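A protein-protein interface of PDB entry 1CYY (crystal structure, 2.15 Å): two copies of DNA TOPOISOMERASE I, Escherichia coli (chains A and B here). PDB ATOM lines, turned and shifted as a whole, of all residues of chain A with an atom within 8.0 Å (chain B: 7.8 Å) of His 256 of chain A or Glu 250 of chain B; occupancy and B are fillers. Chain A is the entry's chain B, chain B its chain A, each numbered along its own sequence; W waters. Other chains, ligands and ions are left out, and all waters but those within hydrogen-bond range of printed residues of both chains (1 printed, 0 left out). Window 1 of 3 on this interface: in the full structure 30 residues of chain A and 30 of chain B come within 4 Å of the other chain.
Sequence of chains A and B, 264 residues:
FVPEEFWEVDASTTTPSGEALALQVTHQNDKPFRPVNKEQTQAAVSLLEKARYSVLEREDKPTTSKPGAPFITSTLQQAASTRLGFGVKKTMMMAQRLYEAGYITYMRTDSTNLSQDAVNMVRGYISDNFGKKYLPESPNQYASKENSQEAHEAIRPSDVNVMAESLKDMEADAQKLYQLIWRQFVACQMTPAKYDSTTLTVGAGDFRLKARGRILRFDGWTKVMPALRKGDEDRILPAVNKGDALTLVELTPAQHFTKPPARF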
ATOM      1  N   PHE A   1      16.178  -0.485  -9.422  1.00  0.00           N
ATOM      2  CA  PHE A   1      17.452   0.239  -9.692  1.00  0.00           C
ATOM      3  C   PHE A   1      17.368   1.019 -10.990  1.00  0.00           C
ATOM      4  O   PHE A   1      16.510   0.758 -11.825  1.00  0.00           O
ATOM      5  CB  PHE A   1      18.637  -0.737  -9.748  1.00  0.00           C
ATOM      6  CG  PHE A   1      19.227  -1.053  -8.403  1.00  0.00           C
ATOM      7  CD1 PHE A   1      20.568  -1.414  -8.291  1.00  0.00           C
ATOM      8  CD2 PHE A   1      18.454  -0.973  -7.248  1.00  0.00           C
ATOM      9  CE1 PHE A   1      21.132  -1.686  -7.049  1.00  0.00           C
ATOM     10  CE2 PHE A   1      19.006  -1.242  -5.997  1.00  0.00           C
ATOM     11  CZ  PHE A   1      20.346  -1.598  -5.897  1.00  0.00           C
ATOM     12  N   VAL A   2      18.274   1.971 -11.158  1.00  0.00           N
ATOM     13  CA  VAL A   2      18.283   2.812 -12.345  1.00  0.00           C
ATOM     14  C   VAL A   2      19.322   2.418 -13.377  1.00  0.00           C
ATOM     15  O   VAL A   2      20.519   2.511 -13.127  1.00  0.00           O
ATOM     16  CB  VAL A   2      18.539   4.285 -11.978  1.00  0.00           C
ATOM     17  CG1 VAL A   2      18.461   5.151 -13.227  1.00  0.00           C
ATOM     18  CG2 VAL A   2      17.533   4.741 -10.924  1.00  0.00           C
ATOM     19  N   PRO A   3      18.874   1.985 -14.563  1.00  0.00           N
ATOM     20  CA  PRO A   3      19.830   1.600 -15.598  1.00  0.00           C
ATOM     21  C   PRO A   3      20.454   2.864 -16.167  1.00  0.00           C
ATOM     22  O   PRO A   3      19.782   3.884 -16.300  1.00  0.00           O
ATOM     23  CB  PRO A   3      18.959   0.861 -16.612  1.00  0.00           C
ATOM     24  CG  PRO A   3      17.666   1.592 -16.523  1.00  0.00           C
ATOM     25  CD  PRO A   3      17.487   1.779 -15.024  1.00  0.00           C
ATOM     26  N   GLU A   4      21.744   2.810 -16.473  1.00  0.00           N
ATOM     27  CA  GLU A   4      22.412   3.969 -17.038  1.00  0.00           C
ATOM     28  C   GLU A   4      21.768   4.193 -18.392  1.00  0.00           C
ATOM     29  O   GLU A   4      21.206   3.265 -18.970  1.00  0.00           O
ATOM     30  CB  GLU A   4      23.904   3.703 -17.184  1.00  0.00           C
ATOM     31  CG  GLU A   4      24.760   4.658 -16.377  1.00  0.00           C
ATOM     32  CD  GLU A   4      26.226   4.283 -16.402  1.00  0.00           C
ATOM     33  OE1 GLU A   4      26.798   4.175 -17.511  1.00  0.00           O
ATOM     34  OE2 GLU A   4      26.803   4.100 -15.305  1.00  0.00           O
ATOM     35  N   GLU A   5      21.845   5.412 -18.906  1.00  0.00           N
ATOM     36  CA  GLU A   5      21.208   5.695 -20.180  1.00  0.00           C
ATOM     37  C   GLU A   5      21.897   5.061 -21.377  1.00  0.00           C
ATOM     38  O   GLU A   5      21.274   4.851 -22.414  1.00  0.00           O
ATOM     39  CB  GLU A   5      21.074   7.205 -20.387  1.00  0.00           C
ATOM     40  CG  GLU A   5      22.327   7.921 -20.836  1.00  0.00           C
ATOM     41  CD  GLU A   5      22.061   9.388 -21.153  1.00  0.00           C
ATOM     42  OE1 GLU A   5      21.091   9.672 -21.899  1.00  0.00           O
ATOM     43  OE2 GLU A   5      22.821  10.254 -20.660  1.00  0.00           O
ATOM     44  N   PHE A   6      23.177   4.746 -21.234  1.00  0.00           N
ATOM     45  CA  PHE A   6      23.924   4.144 -22.332  1.00  0.00           C
ATOM     46  C   PHE A   6      24.649   2.870 -21.942  1.00  0.00           C
ATOM     47  O   PHE A   6      25.184   2.760 -20.844  1.00  0.00           O
ATOM     48  CB  PHE A   6      24.954   5.132 -22.873  1.00  0.00           C
ATOM     49  CG  PHE A   6      24.354   6.387 -23.420  1.00  0.00           C
ATOM     50  CD1 PHE A   6      24.876   7.626 -23.071  1.00  0.00           C
ATOM     51  CD2 PHE A   6      23.267   6.333 -24.285  1.00  0.00           C
ATOM     52  CE1 PHE A   6      24.321   8.795 -23.573  1.00  0.00           C
ATOM     53  CE2 PHE A   6      22.705   7.496 -24.794  1.00  0.00           C
ATOM     54  CZ  PHE A   6      23.232   8.730 -24.437  1.00  0.00           C
ATOM     55  N   TRP A   7      24.658   1.902 -22.844  1.00  0.00           N
ATOM     56  CA  TRP A   7      25.373   0.661 -22.594  1.00  0.00           C
ATOM     57  C   TRP A   7      26.822   1.004 -22.884  1.00  0.00           C
ATOM     58  O   TRP A   7      27.135   2.110 -23.321  1.00  0.00           O
ATOM     59  CB  TRP A   7      24.944  -0.428 -23.574  1.00  0.00           C
ATOM     60  CG  TRP A   7      23.650  -1.087 -23.270  1.00  0.00           C
ATOM     61  CD1 TRP A   7      22.422  -0.495 -23.179  1.00  0.00           C
ATOM     62  CD2 TRP A   7      23.444  -2.484 -23.027  1.00  0.00           C
ATOM     63  NE1 TRP A   7      21.462  -1.440 -22.895  1.00  0.00           N
ATOM     64  CE2 TRP A   7      22.063  -2.667 -22.797  1.00  0.00           C
ATOM     65  CE3 TRP A   7      24.292  -3.596 -22.983  1.00  0.00           C
ATOM     66  CZ2 TRP A   7      21.510  -3.924 -22.524  1.00  0.00           C
ATOM     67  CZ3 TRP A   7      23.745  -4.844 -22.712  1.00  0.00           C
ATOM     68  CH2 TRP A   7      22.365  -4.998 -22.485  1.00  0.00           C
ATOM     69  N   GLU A   8      27.714   0.067 -22.615  1.00  0.00           N
ATOM     70  CA  GLU A   8      29.105   0.279 -22.955  1.00  0.00           C
ATOM     71  C   GLU A   8      29.686  -1.032 -23.421  1.00  0.00           C
ATOM     72  O   GLU A   8      29.116  -2.091 -23.177  1.00  0.00           O
ATOM     73  CB  GLU A   8      29.904   0.900 -21.800  1.00  0.00           C
ATOM     74  CG  GLU A   8      29.950   0.187 -20.474  1.00  0.00           C
ATOM     75  CD  GLU A   8      30.253   1.182 -19.341  1.00  0.00           C
ATOM     76  OE1 GLU A   8      30.847   0.782 -18.316  1.00  0.00           O
ATOM     77  OE2 GLU A   8      29.884   2.378 -19.483  1.00  0.00           O
ATOM     78  N   ASP A  10      33.281  -3.198 -23.553  1.00  0.00           N
ATOM     79  CA  ASP A  10      34.653  -3.352 -23.105  1.00  0.00           C
ATOM     80  C   ASP A  10      35.368  -4.361 -23.976  1.00  0.00           C
ATOM     81  O   ASP A  10      34.742  -5.258 -24.546  1.00  0.00           O
ATOM     82  CB  ASP A  10      34.684  -3.826 -21.654  1.00  0.00           C
ATOM     83  CG  ASP A  10      33.905  -2.907 -20.734  1.00  0.00           C
ATOM     84  OD1 ASP A  10      34.080  -1.677 -20.837  1.00  0.00           O
ATOM     85  OD2 ASP A  10      33.114  -3.412 -19.913  1.00  0.00           O
ATOM     86  N   GLN A  24      37.847   0.286 -22.885  1.00  0.00           N
ATOM     87  CA  GLN A  24      36.441   0.643 -23.004  1.00  0.00           C
ATOM     88  C   GLN A  24      36.291   1.470 -24.283  1.00  0.00           C
ATOM     89  O   GLN A  24      37.111   2.345 -24.562  1.00  0.00           O
ATOM     90  CB  GLN A  24      35.967   1.447 -21.791  1.00  0.00           C
ATOM     91  CG  GLN A  24      34.446   1.554 -21.718  1.00  0.00           C
ATOM     92  CD  GLN A  24      33.957   2.563 -20.690  1.00  0.00           C
ATOM     93  OE1 GLN A  24      34.456   2.610 -19.563  1.00  0.00           O
ATOM     94  NE2 GLN A  24      32.961   3.367 -21.070  1.00  0.00           N
ATOM     95  N   THR A  82      23.509   4.965   0.305  1.00  0.00           N
ATOM     96  CA  THR A  82      24.580   4.200  -0.315  1.00  0.00           C
ATOM     97  C   THR A  82      25.405   3.356   0.663  1.00  0.00           C
ATOM     98  O   THR A  82      25.512   2.136   0.513  1.00  0.00           O
ATOM     99  CB  THR A  82      25.553   5.144  -1.070  1.00  0.00           C
ATOM    100  OG1 THR A  82      24.829   5.941  -2.017  1.00  0.00           O
ATOM    101  CG2 THR A  82      26.611   4.343  -1.812  1.00  0.00           C
ATOM    102  N   ALA A 254      27.960  -4.283 -21.926  1.00  0.00           N
ATOM    103  CA  ALA A 254      27.543  -4.269 -20.528  1.00  0.00           C
ATOM    104  C   ALA A 254      26.716  -3.031 -20.189  1.00  0.00           C
ATOM    105  O   ALA A 254      26.826  -2.013 -20.851  1.00  0.00           O
ATOM    106  CB  ALA A 254      28.779  -4.323 -19.620  1.00  0.00           C
ATOM    107  N   GLN A 255      25.884  -3.130 -19.159  1.00  0.00           N
ATOM    108  CA  GLN A 255      25.081  -1.998 -18.721  1.00  0.00           C
ATOM    109  C   GLN A 255      25.102  -1.964 -17.204  1.00  0.00           C
ATOM    110  O   GLN A 255      25.225  -2.998 -16.566  1.00  0.00           O
ATOM    111  CB  GLN A 255      23.623  -2.093 -19.237  1.00  0.00           C
ATOM    112  CG  GLN A 255      22.871  -3.363 -18.856  1.00  0.00           C
ATOM    113  CD  GLN A 255      21.366  -3.336 -19.210  1.00  0.00           C
ATOM    114  OE1 GLN A 255      20.679  -4.356 -19.075  1.00  0.00           O
ATOM    115  NE2 GLN A 255      20.857  -2.174 -19.645  1.00  0.00           N
ATOM    116  N   HIS A 256      24.997  -0.773 -16.627  1.00  0.00           N
ATOM    117  CA  HIS A 256      25.015  -0.627 -15.177  1.00  0.00           C
ATOM    118  C   HIS A 256      23.639  -0.263 -14.637  1.00  0.00           C
ATOM    119  O   HIS A 256      22.915   0.525 -15.242  1.00  0.00           O
ATOM    120  CB  HIS A 256      26.004   0.463 -14.775  1.00  0.00           C
ATOM    121  CG  HIS A 256      27.400   0.228 -15.265  1.00  0.00           C
ATOM    122  ND1 HIS A 256      28.253  -0.681 -14.675  1.00  0.00           N
ATOM    123  CD2 HIS A 256      28.093   0.785 -16.286  1.00  0.00           C
ATOM    124  CE1 HIS A 256      29.413  -0.672 -15.309  1.00  0.00           C
ATOM    125  NE2 HIS A 256      29.342   0.209 -16.290  1.00  0.00           N
ATOM    126  N   PHE A 257      23.284  -0.857 -13.505  1.00  0.00           N
ATOM    127  CA  PHE A 257      22.025  -0.579 -12.840  1.00  0.00           C
ATOM    128  C   PHE A 257      22.424  -0.040 -11.473  1.00  0.00           C
ATOM    129  O   PHE A 257      23.069  -0.741 -10.690  1.00  0.00           O
ATOM    130  CB  PHE A 257      21.190  -1.853 -12.683  1.00  0.00           C
ATOM    131  CG  PHE A 257      20.573  -2.338 -13.966  1.00  0.00           C
ATOM    132  CD1 PHE A 257      21.326  -3.052 -14.896  1.00  0.00           C
ATOM    133  CD2 PHE A 257      19.237  -2.057 -14.260  1.00  0.00           C
ATOM    134  CE1 PHE A 257      20.760  -3.478 -16.101  1.00  0.00           C
ATOM    135  CE2 PHE A 257      18.658  -2.475 -15.464  1.00  0.00           C
ATOM    136  CZ  PHE A 257      19.423  -3.188 -16.387  1.00  0.00           C
ATOM    137  N   THR A 258      22.051   1.202 -11.186  1.00  0.00           N
ATOM    138  CA  THR A 258      22.422   1.813  -9.912  1.00  0.00           C
ATOM    139  C   THR A 258      21.243   2.147  -9.021  1.00  0.00           C
ATOM    140  O   THR A 258      20.188   2.584  -9.497  1.00  0.00           O
ATOM    141  CB  THR A 258      23.233   3.096 -10.136  1.00  0.00           C
ATOM    142  OG1 THR A 258      22.427   4.042 -10.842  1.00  0.00           O
ATOM    143  CG2 THR A 258      24.477   2.800 -10.963  1.00  0.00           C
ATOM    144  N   LYS A 259      21.430   1.941  -7.721  1.00  0.00           N
ATOM    145  CA  LYS A 259      20.379   2.227  -6.760  1.00  0.00           C
ATOM    146  C   LYS A 259      19.914   3.662  -6.937  1.00  0.00           C
ATOM    147  O   LYS A 259      20.723   4.587  -7.012  1.00  0.00           O
ATOM    148  CB  LYS A 259      20.859   2.018  -5.321  1.00  0.00           C
ATOM    149  CG  LYS A 259      19.966   2.744  -4.318  1.00  0.00           C
ATOM    150  CD  LYS A 259      19.628   1.927  -3.089  1.00  0.00           C
ATOM    151  CE  LYS A 259      20.715   1.999  -2.045  1.00  0.00           C
ATOM    152  NZ  LYS A 259      20.187   1.504  -0.740  1.00  0.00           N
ATOM    153  N   VAL B   9      27.084 -11.403 -14.058  1.00  0.00           N
ATOM    154  CA  VAL B   9      26.595 -10.237 -13.330  1.00  0.00           C
ATOM    155  C   VAL B   9      27.520  -9.945 -12.157  1.00  0.00           C
ATOM    156  O   VAL B   9      27.780 -10.817 -11.330  1.00  0.00           O
ATOM    157  CB  VAL B   9      25.149 -10.439 -12.800  1.00  0.00           C
ATOM    158  CG1 VAL B   9      24.710  -9.215 -11.980  1.00  0.00           C
ATOM    159  CG2 VAL B   9      24.197 -10.633 -13.963  1.00  0.00           C
ATOM    160  N   ASP B  10      28.040  -8.727 -12.123  1.00  0.00           N
ATOM    161  CA  ASP B  10      28.913  -8.281 -11.044  1.00  0.00           C
ATOM    162  C   ASP B  10      28.095  -7.326 -10.191  1.00  0.00           C
ATOM    163  O   ASP B  10      27.202  -6.649 -10.697  1.00  0.00           O
ATOM    164  CB  ASP B  10      30.154  -7.570 -11.601  1.00  0.00           C
ATOM    165  CG  ASP B  10      31.109  -8.533 -12.299  1.00  0.00           C
ATOM    166  OD1 ASP B  10      31.126  -9.723 -11.926  1.00  0.00           O
ATOM    167  OD2 ASP B  10      31.857  -8.112 -13.214  1.00  0.00           O
ATOM    168  N   ALA B  11      28.387  -7.291  -8.897  1.00  0.00           N
ATOM    169  CA  ALA B  11      27.661  -6.428  -7.978  1.00  0.00           C
ATOM    170  C   ALA B  11      28.591  -5.605  -7.106  1.00  0.00           C
ATOM    171  O   ALA B  11      29.618  -6.102  -6.627  1.00  0.00           O
ATOM    172  CB  ALA B  11      26.757  -7.265  -7.089  1.00  0.00           C
ATOM    173  N   SER B  12      28.217  -4.348  -6.898  1.00  0.00           N
ATOM    174  CA  SER B  12      28.987  -3.457  -6.041  1.00  0.00           C
ATOM    175  C   SER B  12      28.149  -3.326  -4.786  1.00  0.00           C
ATOM    176  O   SER B  12      26.944  -3.081  -4.855  1.00  0.00           O
ATOM    177  CB  SER B  12      29.179  -2.080  -6.692  1.00  0.00           C
ATOM    178  OG  SER B  12      29.977  -2.187  -7.867  1.00  0.00           O
ATOM    179  N   THR B  13      28.773  -3.535  -3.641  1.00  0.00           N
ATOM    180  CA  THR B  13      28.055  -3.429  -2.389  1.00  0.00           C
ATOM    181  C   THR B  13      28.885  -2.631  -1.411  1.00  0.00           C
ATOM    182  O   THR B  13      30.059  -2.348  -1.659  1.00  0.00           O
ATOM    183  CB  THR B  13      27.772  -4.816  -1.765  1.00  0.00           C
ATOM    184  OG1 THR B  13      28.996  -5.387  -1.289  1.00  0.00           O
ATOM    185  CG2 THR B  13      27.140  -5.755  -2.796  1.00  0.00           C
ATOM    186  N   THR B  14      28.262  -2.280  -0.297  1.00  0.00           N
ATOM    187  CA  THR B  14      28.909  -1.533   0.764  1.00  0.00           C
ATOM    188  C   THR B  14      28.867  -2.366   2.047  1.00  0.00           C
ATOM    189  O   THR B  14      27.815  -2.886   2.414  1.00  0.00           O
ATOM    190  CB  THR B  14      28.183  -0.192   1.001  1.00  0.00           C
ATOM    191  OG1 THR B  14      28.556   0.742  -0.023  1.00  0.00           O
ATOM    192  CG2 THR B  14      28.554   0.371   2.338  1.00  0.00           C
ATOM    193  N   LEU B  21      32.852  -3.207  -1.651  1.00  0.00           N
ATOM    194  CA  LEU B  21      33.142  -4.628  -1.836  1.00  0.00           C
ATOM    195  C   LEU B  21      32.510  -5.128  -3.139  1.00  0.00           C
ATOM    196  O   LEU B  21      31.273  -5.209  -3.262  1.00  0.00           O
ATOM    197  CB  LEU B  21      32.608  -5.434  -0.650  1.00  0.00           C
ATOM    198  CG  LEU B  21      32.677  -6.963  -0.775  1.00  0.00           C
ATOM    199  CD1 LEU B  21      34.123  -7.433  -0.919  1.00  0.00           C
ATOM    200  CD2 LEU B  21      32.032  -7.591   0.440  1.00  0.00           C
ATOM    201  N   LEU B  23      31.590  -7.943  -5.883  1.00  0.00           N
ATOM    202  CA  LEU B  23      31.299  -9.362  -5.891  1.00  0.00           C
ATOM    203  C   LEU B  23      30.875  -9.795  -7.282  1.00  0.00           C
ATOM    204  O   LEU B  23      30.474  -8.975  -8.098  1.00  0.00           O
ATOM    205  CB  LEU B  23      30.151  -9.663  -4.919  1.00  0.00           C
ATOM    206  CG  LEU B  23      30.291  -9.243  -3.456  1.00  0.00           C
ATOM    207  CD1 LEU B  23      28.900  -9.213  -2.788  1.00  0.00           C
ATOM    208  CD2 LEU B  23      31.240 -10.212  -2.738  1.00  0.00           C
ATOM    209  N   VAL B  45      18.644  -9.768 -12.540  1.00  0.00           N
ATOM    210  CA  VAL B  45      18.975  -8.473 -11.956  1.00  0.00           C
ATOM    211  C   VAL B  45      17.817  -7.954 -11.079  1.00  0.00           C
ATOM    212  O   VAL B  45      18.041  -7.492  -9.950  1.00  0.00           O
ATOM    213  CB  VAL B  45      19.317  -7.443 -13.052  1.00  0.00           C
ATOM    214  CG1 VAL B  45      19.278  -6.021 -12.482  1.00  0.00           C
ATOM    215  CG2 VAL B  45      20.711  -7.741 -13.627  1.00  0.00           C
ATOM    216  N   GLU B  49      18.220  -7.069  -7.266  1.00  0.00           N
ATOM    217  CA  GLU B  49      17.919  -5.723  -6.778  1.00  0.00           C
ATOM    218  C   GLU B  49      17.117  -5.734  -5.475  1.00  0.00           C
ATOM    219  O   GLU B  49      17.325  -4.895  -4.599  1.00  0.00           O
ATOM    220  CB  GLU B  49      17.101  -4.956  -7.814  1.00  0.00           C
ATOM    221  CG  GLU B  49      17.870  -4.439  -9.002  1.00  0.00           C
ATOM    222  CD  GLU B  49      16.945  -3.812 -10.031  1.00  0.00           C
ATOM    223  OE1 GLU B  49      15.830  -3.397  -9.641  1.00  0.00           O
ATOM    224  OE2 GLU B  49      17.328  -3.729 -11.223  1.00  0.00           O
ATOM    225  N   TYR B  53      21.382  -8.840   1.221  1.00  0.00           N
ATOM    226  CA  TYR B  53      22.709  -9.450   1.150  1.00  0.00           C
ATOM    227  C   TYR B  53      23.371  -9.607   2.520  1.00  0.00           C
ATOM    228  O   TYR B  53      23.324  -8.701   3.344  1.00  0.00           O
ATOM    229  CB  TYR B  53      23.627  -8.602   0.258  1.00  0.00           C
ATOM    230  CG  TYR B  53      23.191  -8.488  -1.186  1.00  0.00           C
ATOM    231  CD1 TYR B  53      21.925  -8.000  -1.527  1.00  0.00           C
ATOM    232  CD2 TYR B  53      24.039  -8.883  -2.217  1.00  0.00           C
ATOM    233  CE1 TYR B  53      21.518  -7.921  -2.859  1.00  0.00           C
ATOM    234  CE2 TYR B  53      23.644  -8.806  -3.548  1.00  0.00           C
ATOM    235  CZ  TYR B  53      22.385  -8.332  -3.868  1.00  0.00           C
ATOM    236  OH  TYR B  53      21.981  -8.306  -5.190  1.00  0.00           O
ATOM    237  N   LEU B 209      27.042 -15.031  -4.121  1.00  0.00           N
ATOM    238  CA  LEU B 209      28.048 -14.202  -4.778  1.00  0.00           C
ATOM    239  C   LEU B 209      29.379 -14.444  -4.068  1.00  0.00           C
ATOM    240  O   LEU B 209      29.401 -14.946  -2.944  1.00  0.00           O
ATOM    241  CB  LEU B 209      27.682 -12.715  -4.694  1.00  0.00           C
ATOM    242  CG  LEU B 209      26.330 -12.282  -5.259  1.00  0.00           C
ATOM    243  CD1 LEU B 209      25.250 -12.510  -4.194  1.00  0.00           C
ATOM    244  CD2 LEU B 209      26.380 -10.801  -5.667  1.00  0.00           C
ATOM    245  N   THR B 247      25.063  -3.593   1.630  1.00  0.00           N
ATOM    246  CA  THR B 247      24.079  -2.768   0.934  1.00  0.00           C
ATOM    247  C   THR B 247      24.423  -2.819  -0.551  1.00  0.00           C
ATOM    248  O   THR B 247      25.546  -2.513  -0.939  1.00  0.00           O
ATOM    249  CB  THR B 247      24.138  -1.279   1.377  1.00  0.00           C
ATOM    250  OG1 THR B 247      23.973  -1.180   2.795  1.00  0.00           O
ATOM    251  CG2 THR B 247      23.037  -0.488   0.701  1.00  0.00           C
ATOM    252  N   LEU B 248      23.466  -3.214  -1.381  1.00  0.00           N
ATOM    253  CA  LEU B 248      23.719  -3.287  -2.808  1.00  0.00           C
ATOM    254  C   LEU B 248      23.670  -1.884  -3.372  1.00  0.00           C
ATOM    255  O   LEU B 248      22.727  -1.132  -3.122  1.00  0.00           O
ATOM    256  CB  LEU B 248      22.672  -4.145  -3.516  1.00  0.00           C
ATOM    257  CG  LEU B 248      22.816  -4.180  -5.039  1.00  0.00           C
ATOM    258  CD1 LEU B 248      24.027  -5.049  -5.416  1.00  0.00           C
ATOM    259  CD2 LEU B 248      21.546  -4.739  -5.670  1.00  0.00           C
ATOM    260  N   VAL B 249      24.683  -1.540  -4.155  1.00  0.00           N
ATOM    261  CA  VAL B 249      24.750  -0.226  -4.746  1.00  0.00           C
ATOM    262  C   VAL B 249      24.673  -0.247  -6.264  1.00  0.00           C
ATOM    263  O   VAL B 249      24.179   0.692  -6.877  1.00  0.00           O
ATOM    264  CB  VAL B 249      26.044   0.483  -4.278  1.00  0.00           C
ATOM    265  CG1 VAL B 249      26.606   1.357  -5.379  1.00  0.00           C
ATOM    266  CG2 VAL B 249      25.737   1.316  -3.031  1.00  0.00           C
ATOM    267  N   GLU B 250      25.153  -1.321  -6.880  1.00  0.00           N
ATOM    268  CA  GLU B 250      25.130  -1.393  -8.335  1.00  0.00           C
ATOM    269  C   GLU B 250      25.222  -2.835  -8.836  1.00  0.00           C
ATOM    270  O   GLU B 250      25.837  -3.690  -8.203  1.00  0.00           O
ATOM    271  CB  GLU B 250      26.298  -0.561  -8.898  1.00  0.00           C
ATOM    272  CG  GLU B 250      26.365  -0.462 -10.419  1.00  0.00           C
ATOM    273  CD  GLU B 250      27.617   0.273 -10.910  1.00  0.00           C
ATOM    274  OE1 GLU B 250      27.819   0.364 -12.144  1.00  0.00           O
ATOM    275  OE2 GLU B 250      28.404   0.762 -10.067  1.00  0.00           O
ATOM    276  N   LEU B 251      24.573  -3.102  -9.963  1.00  0.00           N
ATOM    277  CA  LEU B 251      24.615  -4.422 -10.587  1.00  0.00           C
ATOM    278  C   LEU B 251      25.045  -4.153 -12.007  1.00  0.00           C
ATOM    279  O   LEU B 251      24.554  -3.222 -12.633  1.00  0.00           O
ATOM    280  CB  LEU B 251      23.242  -5.091 -10.585  1.00  0.00           C
ATOM    281  CG  LEU B 251      22.746  -5.616  -9.240  1.00  0.00           C
ATOM    282  CD1 LEU B 251      21.281  -6.030  -9.384  1.00  0.00           C
ATOM    283  CD2 LEU B 251      23.608  -6.793  -8.784  1.00  0.00           C
ATOM    284  N   THR B 252      25.960  -4.968 -12.512  1.00  0.00           N
ATOM    285  CA  THR B 252      26.472  -4.786 -13.849  1.00  0.00           C
ATOM    286  C   THR B 252      26.423  -6.080 -14.639  1.00  0.00           C
ATOM    287  O   THR B 252      27.257  -6.964 -14.450  1.00  0.00           O
ATOM    288  CB  THR B 252      27.948  -4.300 -13.811  1.00  0.00           C
ATOM    289  OG1 THR B 252      28.009  -3.019 -13.174  1.00  0.00           O
ATOM    290  CG2 THR B 252      28.537  -4.212 -15.229  1.00  0.00           C
ATOM    291  N   PRO B 253      25.409  -6.233 -15.496  1.00  0.00           N
ATOM    292  CA  PRO B 253      25.365  -7.469 -16.276  1.00  0.00           C
ATOM    293  C   PRO B 253      26.197  -7.251 -17.541  1.00  0.00           C
ATOM    294  O   PRO B 253      26.228  -6.149 -18.098  1.00  0.00           O
ATOM    295  CB  PRO B 253      23.874  -7.644 -16.569  1.00  0.00           C
ATOM    296  CG  PRO B 253      23.372  -6.218 -16.635  1.00  0.00           C
ATOM    297  CD  PRO B 253      24.092  -5.570 -15.469  1.00  0.00           C
HETATM  298  O   HOH W   1      20.230  -1.192  -1.989  1.00  0.00           O
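Glu 5 of chain A touches none of the printed residues of chain B. Glu 8 of chain A touches none of the printed residues of chain B. His 256 of chain A touches just these residues of chain B: Glu 250 (2.8 Å), Leu 251 (3.7 Å) and Thr 252 (2.8 Å). Of the printed residues of chain B, Thr 258 of chain A touches Val 249 and Glu 250. Printed residues of chain B within 4 Å of Lys 259 of chain A: Thr 247 (3.8 Å), Leu 248 (3.9 Å) and Val 249 (3.1 Å). Of the printed residues of chain A, Thr 247 of chain B touches Thr 82 (3.6 Å) and Lys 259 (3.8 Å). Of chain A, only His 256 (2.8 Å), Phe 257 (3.2 Å) and Thr 258 (3.8 Å) come within 4 Å of Glu 250 of chain B. Of the printed residues of chain A, Thr 252 of chain B touches Gln 255 and His 256. The nearest residue of chain A that does not touch Glu 250 of chain B is Phe 1 of chain A (4.04 Å).
The backbone NH (N) of Val 249 of chain B is in hydrogen-bond range of the backbone carbonyl oxygen (O) of Ser 12 of chain B (2.8 Å). The backbone NH (N) of Glu 4 of chain A lies within hydrogen-bond range of the backbone carbonyl oxygen (O) of His 256 of chain A, 2.8 Å away. N of Ala 254 of chain A sits at hydrogen-bond distance from O of Glu 8 of chain A, 2.8 Å away. NE2 of His 256 of chain A is in hydrogen-bond range of OE1 of Glu 8 of chain A, 2.6 Å away.
CZ of Phe 1 of chain A touches CD2 of Leu 248 of chain B (3.4 Å). Thr 82 of chain A touches Val 249 of chain B. Ala 254 of chain A touches Pro 253 of chain B. Gln 255 of chain A touches Leu 251 of chain B (O to O, 3.996 Å). Phe 257 of chain A touches Glu 49 of chain B. Phe 257 of chain A touches Glu 250 of chain B. Phe 257 of chain A touches Pro 253 of chain B (CD1 to CD, 3.8 Å). CG2 of Thr 247 of chain B touches NZ of Lys 259 of chain A, at 3.8 Å.
Water W1 lies within hydrogen-bond range of O of Leu 248 of chain B and NZ of Lys 259 of chain A.
Of the 19 printed residues of chain B, 9 touch a printed residue of chain A. Of the 17 printed residues of chain A, 8 touch a printed residue of chain B. Hydrophobic or aromatic side chains of chain A within 4 Å of the printed part of chain B: Phe 1, Ala 254, His 256 and Phe 257. Among the printed residues, no Asp or Glu carboxylate lies within 4 Å of a Lys or Arg side-chain nitrogen of the other chain.
The side-chain hydroxyl (OG1) of Thr 14 of chain B lies within hydrogen-bond range of the backbone carbonyl oxygen (O) of Thr 82 of chain A (3.4 Å). The side-chain carboxylate of Glu 49 of chain B lies within hydrogen-bond range of the backbone NH of Phe 1 of chain A (2.9 Å). O of Val 249 of chain B is in hydrogen-bond range of N of Lys 259 of chain A (3.1 Å). The side-chain carboxylate (OE1) of Glu 250 of chain B is in hydrogen-bond range of a ring nitrogen (ND1) of His 256 of chain A, 2.8 Å away. The backbone carbonyl oxygen (O) of Leu 251 of chain B sits at hydrogen-bond distance from the backbone NH (N) of Phe 257 of chain A, 2.8 Å away. The side-chain hydroxyl (OG1) of Thr 252 of chain B is in hydrogen-bond range of a ring nitrogen (ND1) of His 256 of chain A (2.8 Å). O of Pro 253 of chain B is in hydrogen-bond range of N of Gln 255 of chain A, 3.2 Å away.
Position printed for both chains: 10. Of the 22 pairs that touch across the chains among the printed residues, none has its exchanged pair printed and touching as well.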
